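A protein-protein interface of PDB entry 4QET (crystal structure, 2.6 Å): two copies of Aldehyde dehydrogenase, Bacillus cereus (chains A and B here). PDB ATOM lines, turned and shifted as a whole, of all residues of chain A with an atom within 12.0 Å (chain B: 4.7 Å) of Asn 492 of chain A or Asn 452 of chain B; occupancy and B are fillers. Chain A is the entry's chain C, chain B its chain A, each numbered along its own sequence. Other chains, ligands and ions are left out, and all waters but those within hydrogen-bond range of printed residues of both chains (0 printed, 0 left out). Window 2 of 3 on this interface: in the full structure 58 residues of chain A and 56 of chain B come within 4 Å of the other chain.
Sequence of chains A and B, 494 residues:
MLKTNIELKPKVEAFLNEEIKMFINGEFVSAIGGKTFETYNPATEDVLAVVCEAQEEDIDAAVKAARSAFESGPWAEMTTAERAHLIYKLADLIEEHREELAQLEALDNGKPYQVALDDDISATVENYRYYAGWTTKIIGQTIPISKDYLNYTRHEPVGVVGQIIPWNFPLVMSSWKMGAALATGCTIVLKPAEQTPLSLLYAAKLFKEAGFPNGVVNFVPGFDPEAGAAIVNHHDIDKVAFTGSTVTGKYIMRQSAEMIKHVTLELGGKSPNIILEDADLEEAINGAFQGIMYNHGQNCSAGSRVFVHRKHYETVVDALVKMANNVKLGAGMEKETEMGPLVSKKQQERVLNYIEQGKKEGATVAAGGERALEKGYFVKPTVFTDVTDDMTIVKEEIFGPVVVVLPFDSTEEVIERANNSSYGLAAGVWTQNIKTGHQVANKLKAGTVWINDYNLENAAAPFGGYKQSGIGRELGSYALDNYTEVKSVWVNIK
No position is printed for both chains.
Of the 7 pairs that touch across the chains among the printed residues, none has its exchanged pair printed and touching as well.
Among the printed residues, merely in contact across the chains: Val 489 of chain A with Ile 451 of chain B (3.7 Å) and Trp 490 of chain A with Trp 450 of chain B (3.4 Å).
Hydrophobic or aromatic side chains of chain B within 4 Å of the printed part of chain A: Trp 450 and Ile 451.
Hydrophobic or aromatic side chains of chain A that line the printed part of chain B: Tyr 149, Val 489 and Trp 490.
Among the printed residues, no Asp or Glu carboxylate lies within 4 Å of a Lys or Arg side-chain nitrogen of the other chain.
Of the printed residues of chain B, Tyr 149 of chain A touches Asp 453 (2.9 Å).
Of the printed residues of chain B, Trp 490 of chain A touches Trp 450 (3.4 Å) and Ile 451 (2.8 Å).
Asn 492 of chain A touches three residues of chain B.
Lys 494 of chain A touches none of the printed residues of chain B.
No residue of chain A comes within 4 Å of Val 429 of chain B.
No residue of chain A comes within 4 Å of Trp 430 of chain B.
Gln 432 of chain B touches none of the printed residues of chain A.
Ile 451 of chain B touches just these residues of chain A: Val 489, Trp 490 and Asn 492.
Of the printed residues of chain A, Asn 452 of chain B touches Asn 492.
Asp 453 of chain B touches two residues of chain A.
The nearest printed residue of chain B that does not touch Asn 492 of chain A is Trp 450 of chain B (6.4 Å).
The nearest residue of chain A that does not touch Asn 452 of chain B is Trp 490 of chain A (5.4 Å).
The nearest printed residue of chain A that does not touch Trp 450 of chain B is Ser 488 of chain A (5.3 Å).
The backbone NH of Asn 492 of chain A sits at hydrogen-bond distance from the backbone carbonyl oxygen of Ile 451 of chain B.
OD1 of Asn 492 of chain A sits close to O of Asn 452 of chain B, at 3.4 Å.
The side-chain carboxylate (OD2) of Asp 453 of chain B lies within hydrogen-bond range of the side-chain hydroxyl (OH) of Tyr 149 of chain A (2.9 Å).
The side-chain carboxylate (OD2) of Asp 453 of chain B sits close to the side-chain amide oxygen (OD1) of Asn 492 of chain A (3.1 Å).
The backbone NH of Ile 451 of chain B is in hydrogen-bond range of the backbone carbonyl oxygen of Trp 490 of chain A (2.8 Å).
The backbone NH of Thr 431 of chain B sits at hydrogen-bond distance from the side-chain amide oxygen of Asn 452 of chain B, 2.9 Å away.
N of Lys 494 of chain A lies close to ND2 of Asn 492 of chain A (3.0 Å).
O of Val 429 of chain B lies within hydrogen-bond range of N of Asn 452 of chain B (2.6 Å).
O of Tyr 152 of chain A lies within hydrogen-bond range of N of Val 489 of chain A (2.7 Å).
The backbone NH (N) of Val 429 of chain B lies within hydrogen-bond range of the backbone carbonyl oxygen (O) of Trp 450 of chain B, 2.8 Å away.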
ATOM      1  N   ILE A 143      12.297  -6.986  19.554  1.00  0.00           N
ATOM      2  CA  ILE A 143      13.124  -6.391  20.577  1.00  0.00           C
ATOM      3  C   ILE A 143      13.491  -7.500  21.554  1.00  0.00           C
ATOM      4  O   ILE A 143      12.595  -8.067  22.189  1.00  0.00           O
ATOM      5  CB  ILE A 143      12.353  -5.246  21.286  1.00  0.00           C
ATOM      6  CG1 ILE A 143      11.805  -4.267  20.254  1.00  0.00           C
ATOM      7  CG2 ILE A 143      13.230  -4.509  22.277  1.00  0.00           C
ATOM      8  CD1 ILE A 143      10.733  -3.338  20.805  1.00  0.00           C
ATOM      9  N   ILE A 145      14.262  -8.857  24.879  1.00  0.00           N
ATOM     10  CA  ILE A 145      14.210  -8.301  26.247  1.00  0.00           C
ATOM     11  C   ILE A 145      14.453  -9.409  27.260  1.00  0.00           C
ATOM     12  O   ILE A 145      15.322  -9.315  28.149  1.00  0.00           O
ATOM     13  CB  ILE A 145      12.881  -7.571  26.512  1.00  0.00           C
ATOM     14  CG1 ILE A 145      12.855  -6.261  25.709  1.00  0.00           C
ATOM     15  CG2 ILE A 145      12.694  -7.262  27.980  1.00  0.00           C
ATOM     16  CD1 ILE A 145      11.479  -5.616  25.559  1.00  0.00           C
ATOM     17  N   SER A 146      13.710 -10.488  27.085  1.00  0.00           N
ATOM     18  CA  SER A 146      13.731 -11.582  28.009  1.00  0.00           C
ATOM     19  C   SER A 146      13.268 -12.836  27.245  1.00  0.00           C
ATOM     20  O   SER A 146      12.462 -12.767  26.313  1.00  0.00           O
ATOM     21  CB  SER A 146      12.807 -11.246  29.166  1.00  0.00           C
ATOM     22  OG  SER A 146      12.003 -12.352  29.448  1.00  0.00           O
ATOM     23  N   LYS A 147      13.812 -13.985  27.625  1.00  0.00           N
ATOM     24  CA  LYS A 147      13.471 -15.231  26.957  1.00  0.00           C
ATOM     25  C   LYS A 147      11.980 -15.554  27.105  1.00  0.00           C
ATOM     26  O   LYS A 147      11.454 -16.367  26.344  1.00  0.00           O
ATOM     27  CB  LYS A 147      14.302 -16.387  27.516  1.00  0.00           C
ATOM     28  CG  LYS A 147      13.883 -16.825  28.916  1.00  0.00           C
ATOM     29  CD  LYS A 147      14.860 -17.846  29.505  1.00  0.00           C
ATOM     30  CE  LYS A 147      14.803 -17.882  31.041  1.00  0.00           C
ATOM     31  NZ  LYS A 147      13.452 -18.185  31.589  1.00  0.00           N
ATOM     32  N   ASP A 148      11.326 -14.917  28.082  1.00  0.00           N
ATOM     33  CA  ASP A 148       9.952 -15.227  28.446  1.00  0.00           C
ATOM     34  C   ASP A 148       8.929 -14.576  27.511  1.00  0.00           C
ATOM     35  O   ASP A 148       7.741 -14.825  27.633  1.00  0.00           O
ATOM     36  CB  ASP A 148       9.661 -14.751  29.884  1.00  0.00           C
ATOM     37  CG  ASP A 148      10.233 -15.675  30.979  1.00  0.00           C
ATOM     38  OD1 ASP A 148      10.284 -15.226  32.149  1.00  0.00           O
ATOM     39  OD2 ASP A 148      10.622 -16.839  30.702  1.00  0.00           O
ATOM     40  N   TYR A 149       9.372 -13.711  26.608  1.00  0.00           N
ATOM     41  CA  TYR A 149       8.463 -12.996  25.725  1.00  0.00           C
ATOM     42  C   TYR A 149       8.969 -12.857  24.323  1.00  0.00           C
ATOM     43  O   TYR A 149      10.167 -12.740  24.095  1.00  0.00           O
ATOM     44  CB  TYR A 149       8.245 -11.573  26.227  1.00  0.00           C
ATOM     45  CG  TYR A 149       7.634 -11.586  27.535  1.00  0.00           C
ATOM     46  CD1 TYR A 149       6.258 -11.735  27.661  1.00  0.00           C
ATOM     47  CD2 TYR A 149       8.424 -11.520  28.676  1.00  0.00           C
ATOM     48  CE1 TYR A 149       5.674 -11.792  28.915  1.00  0.00           C
ATOM     49  CE2 TYR A 149       7.863 -11.580  29.945  1.00  0.00           C
ATOM     50  CZ  TYR A 149       6.494 -11.710  30.060  1.00  0.00           C
ATOM     51  OH  TYR A 149       5.932 -11.765  31.301  1.00  0.00           O
ATOM     52  N   LEU A 150       8.037 -12.777  23.389  1.00  0.00           N
ATOM     53  CA  LEU A 150       8.334 -12.161  22.115  1.00  0.00           C
ATOM     54  C   LEU A 150       7.831 -10.695  22.131  1.00  0.00           C
ATOM     55  O   LEU A 150       6.639 -10.414  22.376  1.00  0.00           O
ATOM     56  CB  LEU A 150       7.691 -12.978  21.000  1.00  0.00           C
ATOM     57  CG  LEU A 150       7.529 -12.288  19.652  1.00  0.00           C
ATOM     58  CD1 LEU A 150       8.893 -12.085  19.027  1.00  0.00           C
ATOM     59  CD2 LEU A 150       6.665 -13.209  18.806  1.00  0.00           C
ATOM     60  N   ASN A 151       8.742  -9.758  21.910  1.00  0.00           N
ATOM     61  CA  ASN A 151       8.363  -8.372  21.748  1.00  0.00           C
ATOM     62  C   ASN A 151       8.493  -7.982  20.322  1.00  0.00           C
ATOM     63  O   ASN A 151       9.525  -8.249  19.717  1.00  0.00           O
ATOM     64  CB  ASN A 151       9.260  -7.489  22.556  1.00  0.00           C
ATOM     65  CG  ASN A 151       8.980  -7.621  24.022  1.00  0.00           C
ATOM     66  OD1 ASN A 151       9.598  -8.448  24.703  1.00  0.00           O
ATOM     67  ND2 ASN A 151       8.003  -6.841  24.523  1.00  0.00           N
ATOM     68  N   TYR A 152       7.447  -7.378  19.766  1.00  0.00           N
ATOM     69  CA  TYR A 152       7.559  -6.851  18.424  1.00  0.00           C
ATOM     70  C   TYR A 152       6.655  -5.621  18.278  1.00  0.00           C
ATOM     71  O   TYR A 152       5.671  -5.470  19.041  1.00  0.00           O
ATOM     72  CB  TYR A 152       7.301  -7.925  17.335  1.00  0.00           C
ATOM     73  CG  TYR A 152       5.857  -8.387  17.192  1.00  0.00           C
ATOM     74  CD1 TYR A 152       4.935  -7.680  16.417  1.00  0.00           C
ATOM     75  CD2 TYR A 152       5.414  -9.542  17.834  1.00  0.00           C
ATOM     76  CE1 TYR A 152       3.618  -8.122  16.296  1.00  0.00           C
ATOM     77  CE2 TYR A 152       4.121  -9.997  17.710  1.00  0.00           C
ATOM     78  CZ  TYR A 152       3.224  -9.286  16.949  1.00  0.00           C
ATOM     79  OH  TYR A 152       1.941  -9.753  16.885  1.00  0.00           O
ATOM     80  N   SER A 488       2.988  -1.999  20.095  1.00  0.00           N
ATOM     81  CA  SER A 488       4.000  -2.787  20.755  1.00  0.00           C
ATOM     82  C   SER A 488       3.276  -3.990  21.302  1.00  0.00           C
ATOM     83  O   SER A 488       2.392  -3.836  22.156  1.00  0.00           O
ATOM     84  CB  SER A 488       4.599  -1.992  21.892  1.00  0.00           C
ATOM     85  OG  SER A 488       5.286  -2.874  22.740  1.00  0.00           O
ATOM     86  N   VAL A 489       3.625  -5.166  20.767  1.00  0.00           N
ATOM     87  CA  VAL A 489       2.955  -6.432  21.099  1.00  0.00           C
ATOM     88  C   VAL A 489       3.870  -7.243  21.993  1.00  0.00           C
ATOM     89  O   VAL A 489       5.078  -7.403  21.700  1.00  0.00           O
ATOM     90  CB  VAL A 489       2.563  -7.288  19.834  1.00  0.00           C
ATOM     91  CG1 VAL A 489       1.758  -8.511  20.239  1.00  0.00           C
ATOM     92  CG2 VAL A 489       1.790  -6.460  18.787  1.00  0.00           C
ATOM     93  N   TRP A 490       3.298  -7.748  23.077  1.00  0.00           N
ATOM     94  CA  TRP A 490       3.986  -8.614  24.022  1.00  0.00           C
ATOM     95  C   TRP A 490       3.391 -10.010  23.934  1.00  0.00           C
ATOM     96  O   TRP A 490       2.213 -10.192  24.220  1.00  0.00           O
ATOM     97  CB  TRP A 490       3.747  -8.097  25.419  1.00  0.00           C
ATOM     98  CG  TRP A 490       4.518  -6.824  25.752  1.00  0.00           C
ATOM     99  CD1 TRP A 490       4.281  -5.535  25.270  1.00  0.00           C
ATOM    100  CD2 TRP A 490       5.629  -6.708  26.669  1.00  0.00           C
ATOM    101  NE1 TRP A 490       5.183  -4.649  25.839  1.00  0.00           N
ATOM    102  CE2 TRP A 490       6.014  -5.331  26.697  1.00  0.00           C
ATOM    103  CE3 TRP A 490       6.329  -7.627  27.473  1.00  0.00           C
ATOM    104  CZ2 TRP A 490       7.088  -4.855  27.501  1.00  0.00           C
ATOM    105  CZ3 TRP A 490       7.432  -7.145  28.277  1.00  0.00           C
ATOM    106  CH2 TRP A 490       7.791  -5.774  28.276  1.00  0.00           C
ATOM    107  N   VAL A 491       4.173 -11.002  23.532  1.00  0.00           N
ATOM    108  CA  VAL A 491       3.626 -12.340  23.481  1.00  0.00           C
ATOM    109  C   VAL A 491       4.297 -13.165  24.592  1.00  0.00           C
ATOM    110  O   VAL A 491       5.476 -13.516  24.461  1.00  0.00           O
ATOM    111  CB  VAL A 491       3.876 -12.976  22.098  1.00  0.00           C
ATOM    112  CG1 VAL A 491       3.188 -14.338  21.964  1.00  0.00           C
ATOM    113  CG2 VAL A 491       3.473 -12.000  20.982  1.00  0.00           C
ATOM    114  N   ASN A 492       3.565 -13.458  25.669  1.00  0.00           N
ATOM    115  CA  ASN A 492       4.041 -14.302  26.753  1.00  0.00           C
ATOM    116  C   ASN A 492       4.292 -15.670  26.150  1.00  0.00           C
ATOM    117  O   ASN A 492       3.398 -16.256  25.521  1.00  0.00           O
ATOM    118  CB  ASN A 492       2.938 -14.415  27.809  1.00  0.00           C
ATOM    119  CG  ASN A 492       3.314 -15.269  29.019  1.00  0.00           C
ATOM    120  OD1 ASN A 492       3.233 -14.789  30.142  1.00  0.00           O
ATOM    121  ND2 ASN A 492       3.671 -16.531  28.813  1.00  0.00           N
ATOM    122  N   ILE A 493       5.523 -16.168  26.285  1.00  0.00           N
ATOM    123  CA  ILE A 493       5.827 -17.511  25.813  1.00  0.00           C
ATOM    124  C   ILE A 493       6.435 -18.373  26.939  1.00  0.00           C
ATOM    125  O   ILE A 493       7.040 -19.391  26.666  1.00  0.00           O
ATOM    126  CB  ILE A 493       6.693 -17.464  24.520  1.00  0.00           C
ATOM    127  CG1 ILE A 493       7.997 -16.708  24.777  1.00  0.00           C
ATOM    128  CG2 ILE A 493       5.946 -16.779  23.384  1.00  0.00           C
ATOM    129  CD1 ILE A 493       8.954 -16.649  23.599  1.00  0.00           C
ATOM    130  N   LYS A 494       6.280 -17.945  28.196  1.00  0.00           N
ATOM    131  CA  LYS A 494       6.748 -18.686  29.395  1.00  0.00           C
ATOM    132  C   LYS A 494       6.219 -20.106  29.444  1.00  0.00           C
ATOM    133  O   LYS A 494       5.125 -20.365  28.906  1.00  0.00           O
ATOM    134  CB  LYS A 494       6.192 -18.072  30.664  1.00  0.00           C
ATOM    135  CG  LYS A 494       6.987 -16.993  31.302  1.00  0.00           C
ATOM    136  CD  LYS A 494       6.063 -16.254  32.253  1.00  0.00           C
ATOM    137  CE  LYS A 494       6.717 -15.027  32.869  1.00  0.00           C
ATOM    138  NZ  LYS A 494       6.069 -14.864  34.200  1.00  0.00           N
ATOM    139  OXT LYS A 494       6.838 -20.986  30.076  1.00  0.00           O
ATOM    140  N   VAL B 429      -5.161  -9.635  25.656  1.00  0.00           N
ATOM    141  CA  VAL B 429      -5.883 -10.683  24.985  1.00  0.00           C
ATOM    142  C   VAL B 429      -5.477 -12.007  25.633  1.00  0.00           C
ATOM    143  O   VAL B 429      -4.276 -12.314  25.736  1.00  0.00           O
ATOM    144  CB  VAL B 429      -5.615 -10.732  23.449  1.00  0.00           C
ATOM    145  CG1 VAL B 429      -6.688 -11.560  22.795  1.00  0.00           C
ATOM    146  CG2 VAL B 429      -5.646  -9.355  22.854  1.00  0.00           C
ATOM    147  N   TRP B 430      -6.477 -12.779  26.060  1.00  0.00           N
ATOM    148  CA  TRP B 430      -6.206 -14.083  26.636  1.00  0.00           C
ATOM    149  C   TRP B 430      -6.834 -15.226  25.815  1.00  0.00           C
ATOM    150  O   TRP B 430      -8.069 -15.328  25.726  1.00  0.00           O
ATOM    151  CB  TRP B 430      -6.675 -14.135  28.072  1.00  0.00           C
ATOM    152  CG  TRP B 430      -6.026 -13.129  28.934  1.00  0.00           C
ATOM    153  CD1 TRP B 430      -6.385 -11.811  29.095  1.00  0.00           C
ATOM    154  CD2 TRP B 430      -4.917 -13.354  29.810  1.00  0.00           C
ATOM    155  NE1 TRP B 430      -5.567 -11.206  30.027  1.00  0.00           N
ATOM    156  CE2 TRP B 430      -4.657 -12.126  30.479  1.00  0.00           C
ATOM    157  CE3 TRP B 430      -4.125 -14.487  30.113  1.00  0.00           C
ATOM    158  CZ2 TRP B 430      -3.609 -11.983  31.408  1.00  0.00           C
ATOM    159  CZ3 TRP B 430      -3.089 -14.357  31.051  1.00  0.00           C
ATOM    160  CH2 TRP B 430      -2.836 -13.107  31.684  1.00  0.00           C
ATOM    161  N   THR B 431      -5.983 -16.046  25.203  1.00  0.00           N
ATOM    162  CA  THR B 431      -6.395 -17.086  24.271  1.00  0.00           C
ATOM    163  C   THR B 431      -5.150 -17.907  24.034  1.00  0.00           C
ATOM    164  O   THR B 431      -4.062 -17.344  23.914  1.00  0.00           O
ATOM    165  CB  THR B 431      -6.869 -16.552  22.894  1.00  0.00           C
ATOM    166  OG1 THR B 431      -6.872 -17.631  21.969  1.00  0.00           O
ATOM    167  CG2 THR B 431      -5.896 -15.475  22.323  1.00  0.00           C
ATOM    168  N   GLN B 432      -5.313 -19.228  24.005  1.00  0.00           N
ATOM    169  CA  GLN B 432      -4.208 -20.169  23.795  1.00  0.00           C
ATOM    170  C   GLN B 432      -3.983 -20.388  22.303  1.00  0.00           C
ATOM    171  O   GLN B 432      -3.044 -21.068  21.919  1.00  0.00           O
ATOM    172  CB  GLN B 432      -4.479 -21.500  24.469  1.00  0.00           C
ATOM    173  CG  GLN B 432      -4.409 -21.447  25.982  1.00  0.00           C
ATOM    174  CD  GLN B 432      -2.991 -21.463  26.513  1.00  0.00           C
ATOM    175  OE1 GLN B 432      -2.529 -20.488  27.102  1.00  0.00           O
ATOM    176  NE2 GLN B 432      -2.286 -22.554  26.287  1.00  0.00           N
ATOM    177  N   TRP B 450      -0.871  -6.842  25.125  1.00  0.00           N
ATOM    178  CA  TRP B 450      -0.310  -8.001  25.771  1.00  0.00           C
ATOM    179  C   TRP B 450      -1.184  -9.196  25.401  1.00  0.00           C
ATOM    180  O   TRP B 450      -2.434  -9.138  25.524  1.00  0.00           O
ATOM    181  CB  TRP B 450      -0.325  -7.806  27.278  1.00  0.00           C
ATOM    182  CG  TRP B 450       0.471  -6.587  27.789  1.00  0.00           C
ATOM    183  CD1 TRP B 450       1.832  -6.471  27.861  1.00  0.00           C
ATOM    184  CD2 TRP B 450      -0.066  -5.336  28.304  1.00  0.00           C
ATOM    185  NE1 TRP B 450       2.168  -5.241  28.382  1.00  0.00           N
ATOM    186  CE2 TRP B 450       1.032  -4.542  28.691  1.00  0.00           C
ATOM    187  CE3 TRP B 450      -1.378  -4.827  28.491  1.00  0.00           C
ATOM    188  CZ2 TRP B 450       0.878  -3.246  29.229  1.00  0.00           C
ATOM    189  CZ3 TRP B 450      -1.546  -3.550  29.077  1.00  0.00           C
ATOM    190  CH2 TRP B 450      -0.417  -2.776  29.440  1.00  0.00           C
ATOM    191  N   ILE B 451      -0.552 -10.258  24.884  1.00  0.00           N
ATOM    192  CA  ILE B 451      -1.241 -11.519  24.645  1.00  0.00           C
ATOM    193  C   ILE B 451      -0.840 -12.504  25.755  1.00  0.00           C
ATOM    194  O   ILE B 451       0.352 -12.881  25.884  1.00  0.00           O
ATOM    195  CB  ILE B 451      -0.907 -12.107  23.256  1.00  0.00           C
ATOM    196  CG1 ILE B 451      -1.129 -11.039  22.138  1.00  0.00           C
ATOM    197  CG2 ILE B 451      -1.654 -13.436  23.090  1.00  0.00           C
ATOM    198  CD1 ILE B 451      -0.575 -11.389  20.760  1.00  0.00           C
ATOM    199  N   ASN B 452      -1.828 -12.898  26.560  1.00  0.00           N
ATOM    200  CA  ASN B 452      -1.654 -13.741  27.760  1.00  0.00           C
ATOM    201  C   ASN B 452      -0.781 -13.071  28.797  1.00  0.00           C
ATOM    202  O   ASN B 452       0.064 -13.683  29.457  1.00  0.00           O
ATOM    203  CB  ASN B 452      -1.229 -15.177  27.442  1.00  0.00           C
ATOM    204  CG  ASN B 452      -2.130 -15.829  26.407  1.00  0.00           C
ATOM    205  OD1 ASN B 452      -3.355 -15.738  26.486  1.00  0.00           O
ATOM    206  ND2 ASN B 452      -1.525 -16.429  25.385  1.00  0.00           N
ATOM    207  N   ASP B 453      -1.016 -11.785  28.978  1.00  0.00           N
ATOM    208  CA  ASP B 453      -0.345 -11.076  30.054  1.00  0.00           C
ATOM    209  C   ASP B 453      -0.938  -9.696  30.179  1.00  0.00           C
ATOM    210  O   ASP B 453      -1.826  -9.328  29.420  1.00  0.00           O
ATOM    211  CB  ASP B 453       1.167 -11.016  29.815  1.00  0.00           C
ATOM    212  CG  ASP B 453       1.950 -11.165  31.102  1.00  0.00           C
ATOM    213  OD1 ASP B 453       1.462 -10.645  32.124  1.00  0.00           O
ATOM    214  OD2 ASP B 453       3.033 -11.807  31.101  1.00  0.00           O
